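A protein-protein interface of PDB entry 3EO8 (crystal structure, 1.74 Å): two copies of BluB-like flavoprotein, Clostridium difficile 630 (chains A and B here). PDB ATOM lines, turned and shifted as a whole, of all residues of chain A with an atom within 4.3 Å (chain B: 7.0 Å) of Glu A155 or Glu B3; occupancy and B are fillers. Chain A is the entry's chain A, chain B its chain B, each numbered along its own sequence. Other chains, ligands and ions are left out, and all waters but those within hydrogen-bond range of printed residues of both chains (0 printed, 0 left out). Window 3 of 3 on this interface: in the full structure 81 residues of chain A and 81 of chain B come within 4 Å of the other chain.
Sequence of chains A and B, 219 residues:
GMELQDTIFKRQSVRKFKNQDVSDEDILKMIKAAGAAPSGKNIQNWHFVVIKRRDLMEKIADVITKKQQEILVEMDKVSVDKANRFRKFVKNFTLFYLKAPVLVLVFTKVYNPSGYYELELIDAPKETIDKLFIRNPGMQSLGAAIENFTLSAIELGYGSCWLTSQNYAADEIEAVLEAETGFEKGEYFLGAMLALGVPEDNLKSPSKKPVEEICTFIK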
ATOM      1  N   GLY A   1      26.688 -14.075  12.802  1.00  0.00           N
ATOM      2  CA  GLY A   1      26.584 -12.839  13.628  1.00  0.00           C
ATOM      3  C   GLY A   1      26.518 -11.597  12.757  1.00  0.00           C
ATOM      4  O   GLY A   1      26.513 -11.684  11.523  1.00  0.00           O
ATOM      5  N   MET A   2      26.478 -10.438  13.408  1.00  0.00           N
ATOM      6  CA  MET A   2      26.318  -9.161  12.736  1.00  0.00           C
ATOM      7  C   MET A   2      27.404  -8.223  13.221  1.00  0.00           C
ATOM      8  O   MET A   2      27.756  -8.236  14.403  1.00  0.00           O
ATOM      9  CB  MET A   2      24.943  -8.581  13.045  1.00  0.00           C
ATOM     10  CG  MET A   2      24.512  -7.469  12.141  1.00  0.00           C
ATOM     11  SD  MET A   2      22.638  -7.008  12.436  1.00  0.00           S
ATOM     12  CE  MET A   2      21.948  -8.628  11.863  1.00  0.00           C
ATOM     13  N   GLU A   3      27.953  -7.436  12.303  1.00  0.00           N
ATOM     14  CA  GLU A   3      28.999  -6.473  12.645  1.00  0.00           C
ATOM     15  C   GLU A   3      28.359  -5.324  13.423  1.00  0.00           C
ATOM     16  O   GLU A   3      27.175  -5.016  13.216  1.00  0.00           O
ATOM     17  CB  GLU A   3      29.680  -5.991  11.373  1.00  0.00           C
ATOM     18  CG  GLU A   3      30.760  -4.911  11.561  1.00  0.00           C
ATOM     19  CD  GLU A   3      30.221  -3.482  11.436  1.00  0.00           C
ATOM     20  OE1 GLU A   3      29.155  -3.276  10.813  1.00  0.00           O
ATOM     21  OE2 GLU A   3      30.876  -2.554  11.946  1.00  0.00           O
ATOM     22  N   LEU A 151      20.865  -4.040  20.978  1.00  0.00           N
ATOM     23  CA  LEU A 151      21.698  -4.363  19.842  1.00  0.00           C
ATOM     24  C   LEU A 151      21.750  -5.872  19.628  1.00  0.00           C
ATOM     25  O   LEU A 151      21.773  -6.364  18.485  1.00  0.00           O
ATOM     26  CB  LEU A 151      23.099  -3.762  20.030  1.00  0.00           C
ATOM     27  CG  LEU A 151      23.178  -2.226  20.098  1.00  0.00           C
ATOM     28  CD1 LEU A 151      24.602  -1.820  20.286  1.00  0.00           C
ATOM     29  CD2 LEU A 151      22.548  -1.540  18.811  1.00  0.00           C
ATOM     30  N   SER A 152      21.768  -6.617  20.727  1.00  0.00           N
ATOM     31  CA  SER A 152      21.838  -8.072  20.666  1.00  0.00           C
ATOM     32  C   SER A 152      20.572  -8.664  20.080  1.00  0.00           C
ATOM     33  O   SER A 152      20.629  -9.601  19.284  1.00  0.00           O
ATOM     34  CB  SER A 152      22.110  -8.633  22.063  1.00  0.00           C
ATOM     35  OG  SER A 152      23.341  -8.119  22.543  1.00  0.00           O
ATOM     36  N   ALA A 153      19.439  -8.105  20.476  1.00  0.00           N
ATOM     37  CA  ALA A 153      18.141  -8.479  19.880  1.00  0.00           C
ATOM     38  C   ALA A 153      18.201  -8.366  18.367  1.00  0.00           C
ATOM     39  O   ALA A 153      17.813  -9.295  17.657  1.00  0.00           O
ATOM     40  CB  ALA A 153      17.005  -7.599  20.432  1.00  0.00           C
ATOM     41  N   ILE A 154      18.732  -7.244  17.863  1.00  0.00           N
ATOM     42  CA  ILE A 154      18.841  -7.029  16.398  1.00  0.00           C
ATOM     43  C   ILE A 154      19.771  -8.046  15.721  1.00  0.00           C
ATOM     44  O   ILE A 154      19.425  -8.675  14.692  1.00  0.00           O
ATOM     45  CB  ILE A 154      19.280  -5.567  16.079  1.00  0.00           C
ATOM     46  CG1 ILE A 154      18.210  -4.559  16.526  1.00  0.00           C
ATOM     47  CG2 ILE A 154      19.518  -5.413  14.562  1.00  0.00           C
ATOM     48  CD1 ILE A 154      18.754  -3.197  16.844  1.00  0.00           C
ATOM     49  N   GLU A 155      20.924  -8.304  16.330  1.00  0.00           N
ATOM     50  CA  GLU A 155      21.824  -9.320  15.791  1.00  0.00           C
ATOM     51  C   GLU A 155      21.160 -10.676  15.642  1.00  0.00           C
ATOM     52  O   GLU A 155      21.467 -11.411  14.712  1.00  0.00           O
ATOM     53  CB  GLU A 155      23.072  -9.494  16.654  1.00  0.00           C
ATOM     54  CG  GLU A 155      24.001 -10.544  16.107  1.00  0.00           C
ATOM     55  CD  GLU A 155      25.324 -10.666  16.840  1.00  0.00           C
ATOM     56  OE1 GLU A 155      25.368 -10.396  18.050  1.00  0.00           O
ATOM     57  OE2 GLU A 155      26.320 -11.056  16.181  1.00  0.00           O
ATOM     58  N   LEU A 156      20.287 -11.016  16.584  1.00  0.00           N
ATOM     59  CA  LEU A 156      19.627 -12.327  16.608  1.00  0.00           C
ATOM     60  C   LEU A 156      18.380 -12.412  15.697  1.00  0.00           C
ATOM     61  O   LEU A 156      17.755 -13.480  15.588  1.00  0.00           O
ATOM     62  CB  LEU A 156      19.284 -12.705  18.068  1.00  0.00           C
ATOM     63  CG  LEU A 156      20.527 -13.001  18.936  1.00  0.00           C
ATOM     64  CD1 LEU A 156      20.241 -12.911  20.389  1.00  0.00           C
ATOM     65  CD2 LEU A 156      21.132 -14.379  18.582  1.00  0.00           C
ATOM     66  N   GLY A 157      18.036 -11.313  15.019  1.00  0.00           N
ATOM     67  CA  GLY A 157      16.926 -11.311  14.069  1.00  0.00           C
ATOM     68  C   GLY A 157      15.632 -10.723  14.592  1.00  0.00           C
ATOM     69  O   GLY A 157      14.570 -10.896  13.986  1.00  0.00           O
ATOM     70  N   GLY B   1      35.828  -4.946  10.177  1.00  0.00           N
ATOM     71  CA  GLY B   1      34.787  -4.773  11.230  1.00  0.00           C
ATOM     72  C   GLY B   1      34.895  -5.816  12.329  1.00  0.00           C
ATOM     73  O   GLY B   1      35.742  -6.725  12.244  1.00  0.00           O
ATOM     74  N   MET B   2      34.049  -5.684  13.352  1.00  0.00           N
ATOM     75  CA  MET B   2      34.008  -6.629  14.472  1.00  0.00           C
ATOM     76  C   MET B   2      32.583  -6.995  14.816  1.00  0.00           C
ATOM     77  O   MET B   2      31.694  -6.148  14.784  1.00  0.00           O
ATOM     78  CB  MET B   2      34.701  -6.035  15.693  1.00  0.00           C
ATOM     79  CG  MET B   2      34.899  -6.997  16.850  1.00  0.00           C
ATOM     80  SD  MET B   2      35.874  -6.146  18.345  1.00  0.00           S
ATOM     81  CE  MET B   2      37.335  -5.673  17.381  1.00  0.00           C
ATOM     82  N   GLU B   3      32.371  -8.269  15.137  1.00  0.00           N
ATOM     83  CA  GLU B   3      31.026  -8.789  15.442  1.00  0.00           C
ATOM     84  C   GLU B   3      30.552  -8.255  16.795  1.00  0.00           C
ATOM     85  O   GLU B   3      31.360  -8.021  17.688  1.00  0.00           O
ATOM     86  CB  GLU B   3      31.068 -10.313  15.414  1.00  0.00           C
ATOM     87  CG  GLU B   3      29.739 -11.020  15.676  1.00  0.00           C
ATOM     88  CD  GLU B   3      29.530 -11.322  17.155  1.00  0.00           C
ATOM     89  OE1 GLU B   3      30.533 -11.462  17.887  1.00  0.00           O
ATOM     90  OE2 GLU B   3      28.370 -11.445  17.595  1.00  0.00           O
ATOM     91  N   LEU B   4      29.245  -8.059  16.938  1.00  0.00           N
ATOM     92  CA  LEU B   4      28.676  -7.400  18.102  1.00  0.00           C
ATOM     93  C   LEU B   4      29.049  -8.064  19.430  1.00  0.00           C
ATOM     94  O   LEU B   4      29.571  -7.399  20.325  1.00  0.00           O
ATOM     95  CB  LEU B   4      27.150  -7.320  17.985  1.00  0.00           C
ATOM     96  CG  LEU B   4      26.409  -6.730  19.189  1.00  0.00           C
ATOM     97  CD1 LEU B   4      26.719  -5.273  19.409  1.00  0.00           C
ATOM     98  CD2 LEU B   4      24.904  -6.911  18.989  1.00  0.00           C
ATOM     99  N   GLN B   5      28.772  -9.361  19.567  1.00  0.00           N
ATOM    100  CA  GLN B   5      29.041 -10.028  20.841  1.00  0.00           C
ATOM    101  C   GLN B   5      30.522  -9.962  21.197  1.00  0.00           C
ATOM    102  O   GLN B   5      30.865  -9.754  22.339  1.00  0.00           O
ATOM    103  CB  GLN B   5      28.556 -11.473  20.840  1.00  0.00           C
ATOM    104  CG  GLN B   5      27.055 -11.633  20.696  1.00  0.00           C
ATOM    105  CD  GLN B   5      26.251 -10.749  21.661  1.00  0.00           C
ATOM    106  OE1 GLN B   5      26.369 -10.882  22.877  1.00  0.00           O
ATOM    107  NE2 GLN B   5      25.439  -9.850  21.116  1.00  0.00           N
ATOM    108  N   ASP B   6      31.391 -10.120  20.205  1.00  0.00           N
ATOM    109  CA  ASP B   6      32.823  -9.958  20.418  1.00  0.00           C
ATOM    110  C   ASP B   6      33.186  -8.601  21.060  1.00  0.00           C
ATOM    111  O   ASP B   6      33.969  -8.554  22.022  1.00  0.00           O
ATOM    112  CB  ASP B   6      33.593 -10.189  19.111  1.00  0.00           C
ATOM    113  CG  ASP B   6      33.592 -11.639  18.697  1.00  0.00           C
ATOM    114  OD1 ASP B   6      33.152 -12.493  19.505  1.00  0.00           O
ATOM    115  OD2 ASP B   6      34.022 -11.941  17.559  1.00  0.00           O
ATOM    116  N   THR B   7      32.592  -7.521  20.560  1.00  0.00           N
ATOM    117  CA  THR B   7      32.852  -6.179  21.086  1.00  0.00           C
ATOM    118  C   THR B   7      32.304  -6.059  22.498  1.00  0.00           C
ATOM    119  O   THR B   7      32.980  -5.563  23.394  1.00  0.00           O
ATOM    120  CB  THR B   7      32.248  -5.021  20.214  1.00  0.00           C
ATOM    121  OG1 THR B   7      30.814  -5.039  20.270  1.00  0.00           O
ATOM    122  CG2 THR B   7      32.716  -5.129  18.757  1.00  0.00           C
ATOM    123  N   ILE B   8      31.081  -6.519  22.694  1.00  0.00           N
ATOM    124  CA  ILE B   8      30.432  -6.473  23.998  1.00  0.00           C
ATOM    125  C   ILE B   8      31.232  -7.163  25.121  1.00  0.00           C
ATOM    126  O   ILE B   8      31.367  -6.630  26.229  1.00  0.00           O
ATOM    127  CB  ILE B   8      29.028  -7.103  23.926  1.00  0.00           C
ATOM    128  CG1 ILE B   8      28.093  -6.147  23.175  1.00  0.00           C
ATOM    129  CG2 ILE B   8      28.446  -7.369  25.367  1.00  0.00           C
ATOM    130  CD1 ILE B   8      26.660  -6.626  23.014  1.00  0.00           C
ATOM    131  N   GLU B 155      35.632  -1.663  18.399  1.00  0.00           N
ATOM    132  CA  GLU B 155      35.654  -2.175  17.026  1.00  0.00           C
ATOM    133  C   GLU B 155      36.803  -1.567  16.247  1.00  0.00           C
ATOM    134  O   GLU B 155      37.404  -2.233  15.405  1.00  0.00           O
ATOM    135  CB  GLU B 155      34.357  -1.853  16.300  1.00  0.00           C
ATOM    136  CG  GLU B 155      34.376  -2.217  14.835  1.00  0.00           C
ATOM    137  CD  GLU B 155      33.007  -2.156  14.198  1.00  0.00           C
ATOM    138  OE1 GLU B 155      32.233  -1.239  14.546  1.00  0.00           O
ATOM    139  OE2 GLU B 155      32.750  -3.015  13.320  1.00  0.00           O
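Of the 10 printed residues of chain A, 5 touch a printed residue of chain B. Hydrophobic or aromatic side chains of chain A that line the printed part of chain B: Leu A151. Of the 9 printed residues of chain B, 6 touch a printed residue of chain A. Printed residues of chain B that touch a printed residue of chain A: Met B2, Glu B3, Leu B4, Gln B5, Ile B8 and Glu B155. Hydrophobic or aromatic side chains of chain B within 4 Å of the printed part of chain A: Leu B4 and Ile B8. Among the printed residues, no Asp or Glu carboxylate lies within 4 Å of a Lys or Arg side-chain nitrogen of the other chain.
Met A2 touches Glu B3, and with the chains exchanged Glu A3 touches Met B2. Glu A3 touches Glu B155, and with the chains exchanged Glu A155 touches Glu B3. Of the 11 pairs that touch across the chains among the printed residues, 4 have their exchanged pair printed and touching as well.
CA of Glu B3 touches O of Met A2, at 3.5 Å. Met B2 touches Glu A3. Leu B4 touches Leu A151. Ser A152 touches Leu B4 (N to CD2, 3.6 Å). CD1 of Ile B8 touches OG of Ser A152 (3.7 Å). Glu A155 touches Leu B4 (OE1 to CB, 3.6 Å).
Glu A155 touches three residues of chain B. Printed residues of chain A within 4 Å of Gln B5: Ser A152 and Glu A155. Of the printed residues of chain A, Met B2 touches Glu A3. Printed residues of chain B within 4 Å of Ser A152: Leu B4 (3.6 Å), Gln B5 (3.1 Å) and Ile B8 (3.7 Å). Of the printed residues of chain B, Glu A3 touches Met B2 (3.5 Å) and Glu B155 (2.4 Å). Ile A154 touches none of the printed residues of chain B. Gly B1 touches none of the printed residues of chain A. The nearest residue of chain B that does not touch Glu A155 is Ile B8 (6.4 Å). The nearest printed residue of chain B that does not touch Met A2 is Met B2 (4.5 Å).
The side-chain carboxylate (OE2) of Glu A3 sits close to the side-chain carboxylate (OE2) of Glu B155 (2.4 Å). The side-chain carboxylate (OE1) of Glu A155 sits at hydrogen-bond distance from the side-chain amide nitrogen (NE2) of Gln B5. OE2 of Glu B3 lies close to OE2 of Glu A155, 2.5 Å away. The side-chain amide nitrogen of Gln B5 is in hydrogen-bond range of the side-chain hydroxyl of Ser A152, at 3.1 Å. The backbone NH (N) of Leu B4 lies within hydrogen-bond range of the backbone carbonyl oxygen (O) of Met A2 (2.9 Å).
The backbone NH (N) of Gln B5 is in hydrogen-bond range of the side-chain carboxylate (OE2) of Glu B3, at 2.9 Å. OE2 of Glu A155 is in hydrogen-bond range of N of Met A2, 2.8 Å away. OE2 of Glu B155 sits at hydrogen-bond distance from N of Met B2 (3.0 Å). The backbone NH (N) of Asp B6 lies within hydrogen-bond range of the side-chain carboxylate (OE1) of Glu B3 (2.8 Å). O of Leu B4 is in hydrogen-bond range of OG1 of Thr B7.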
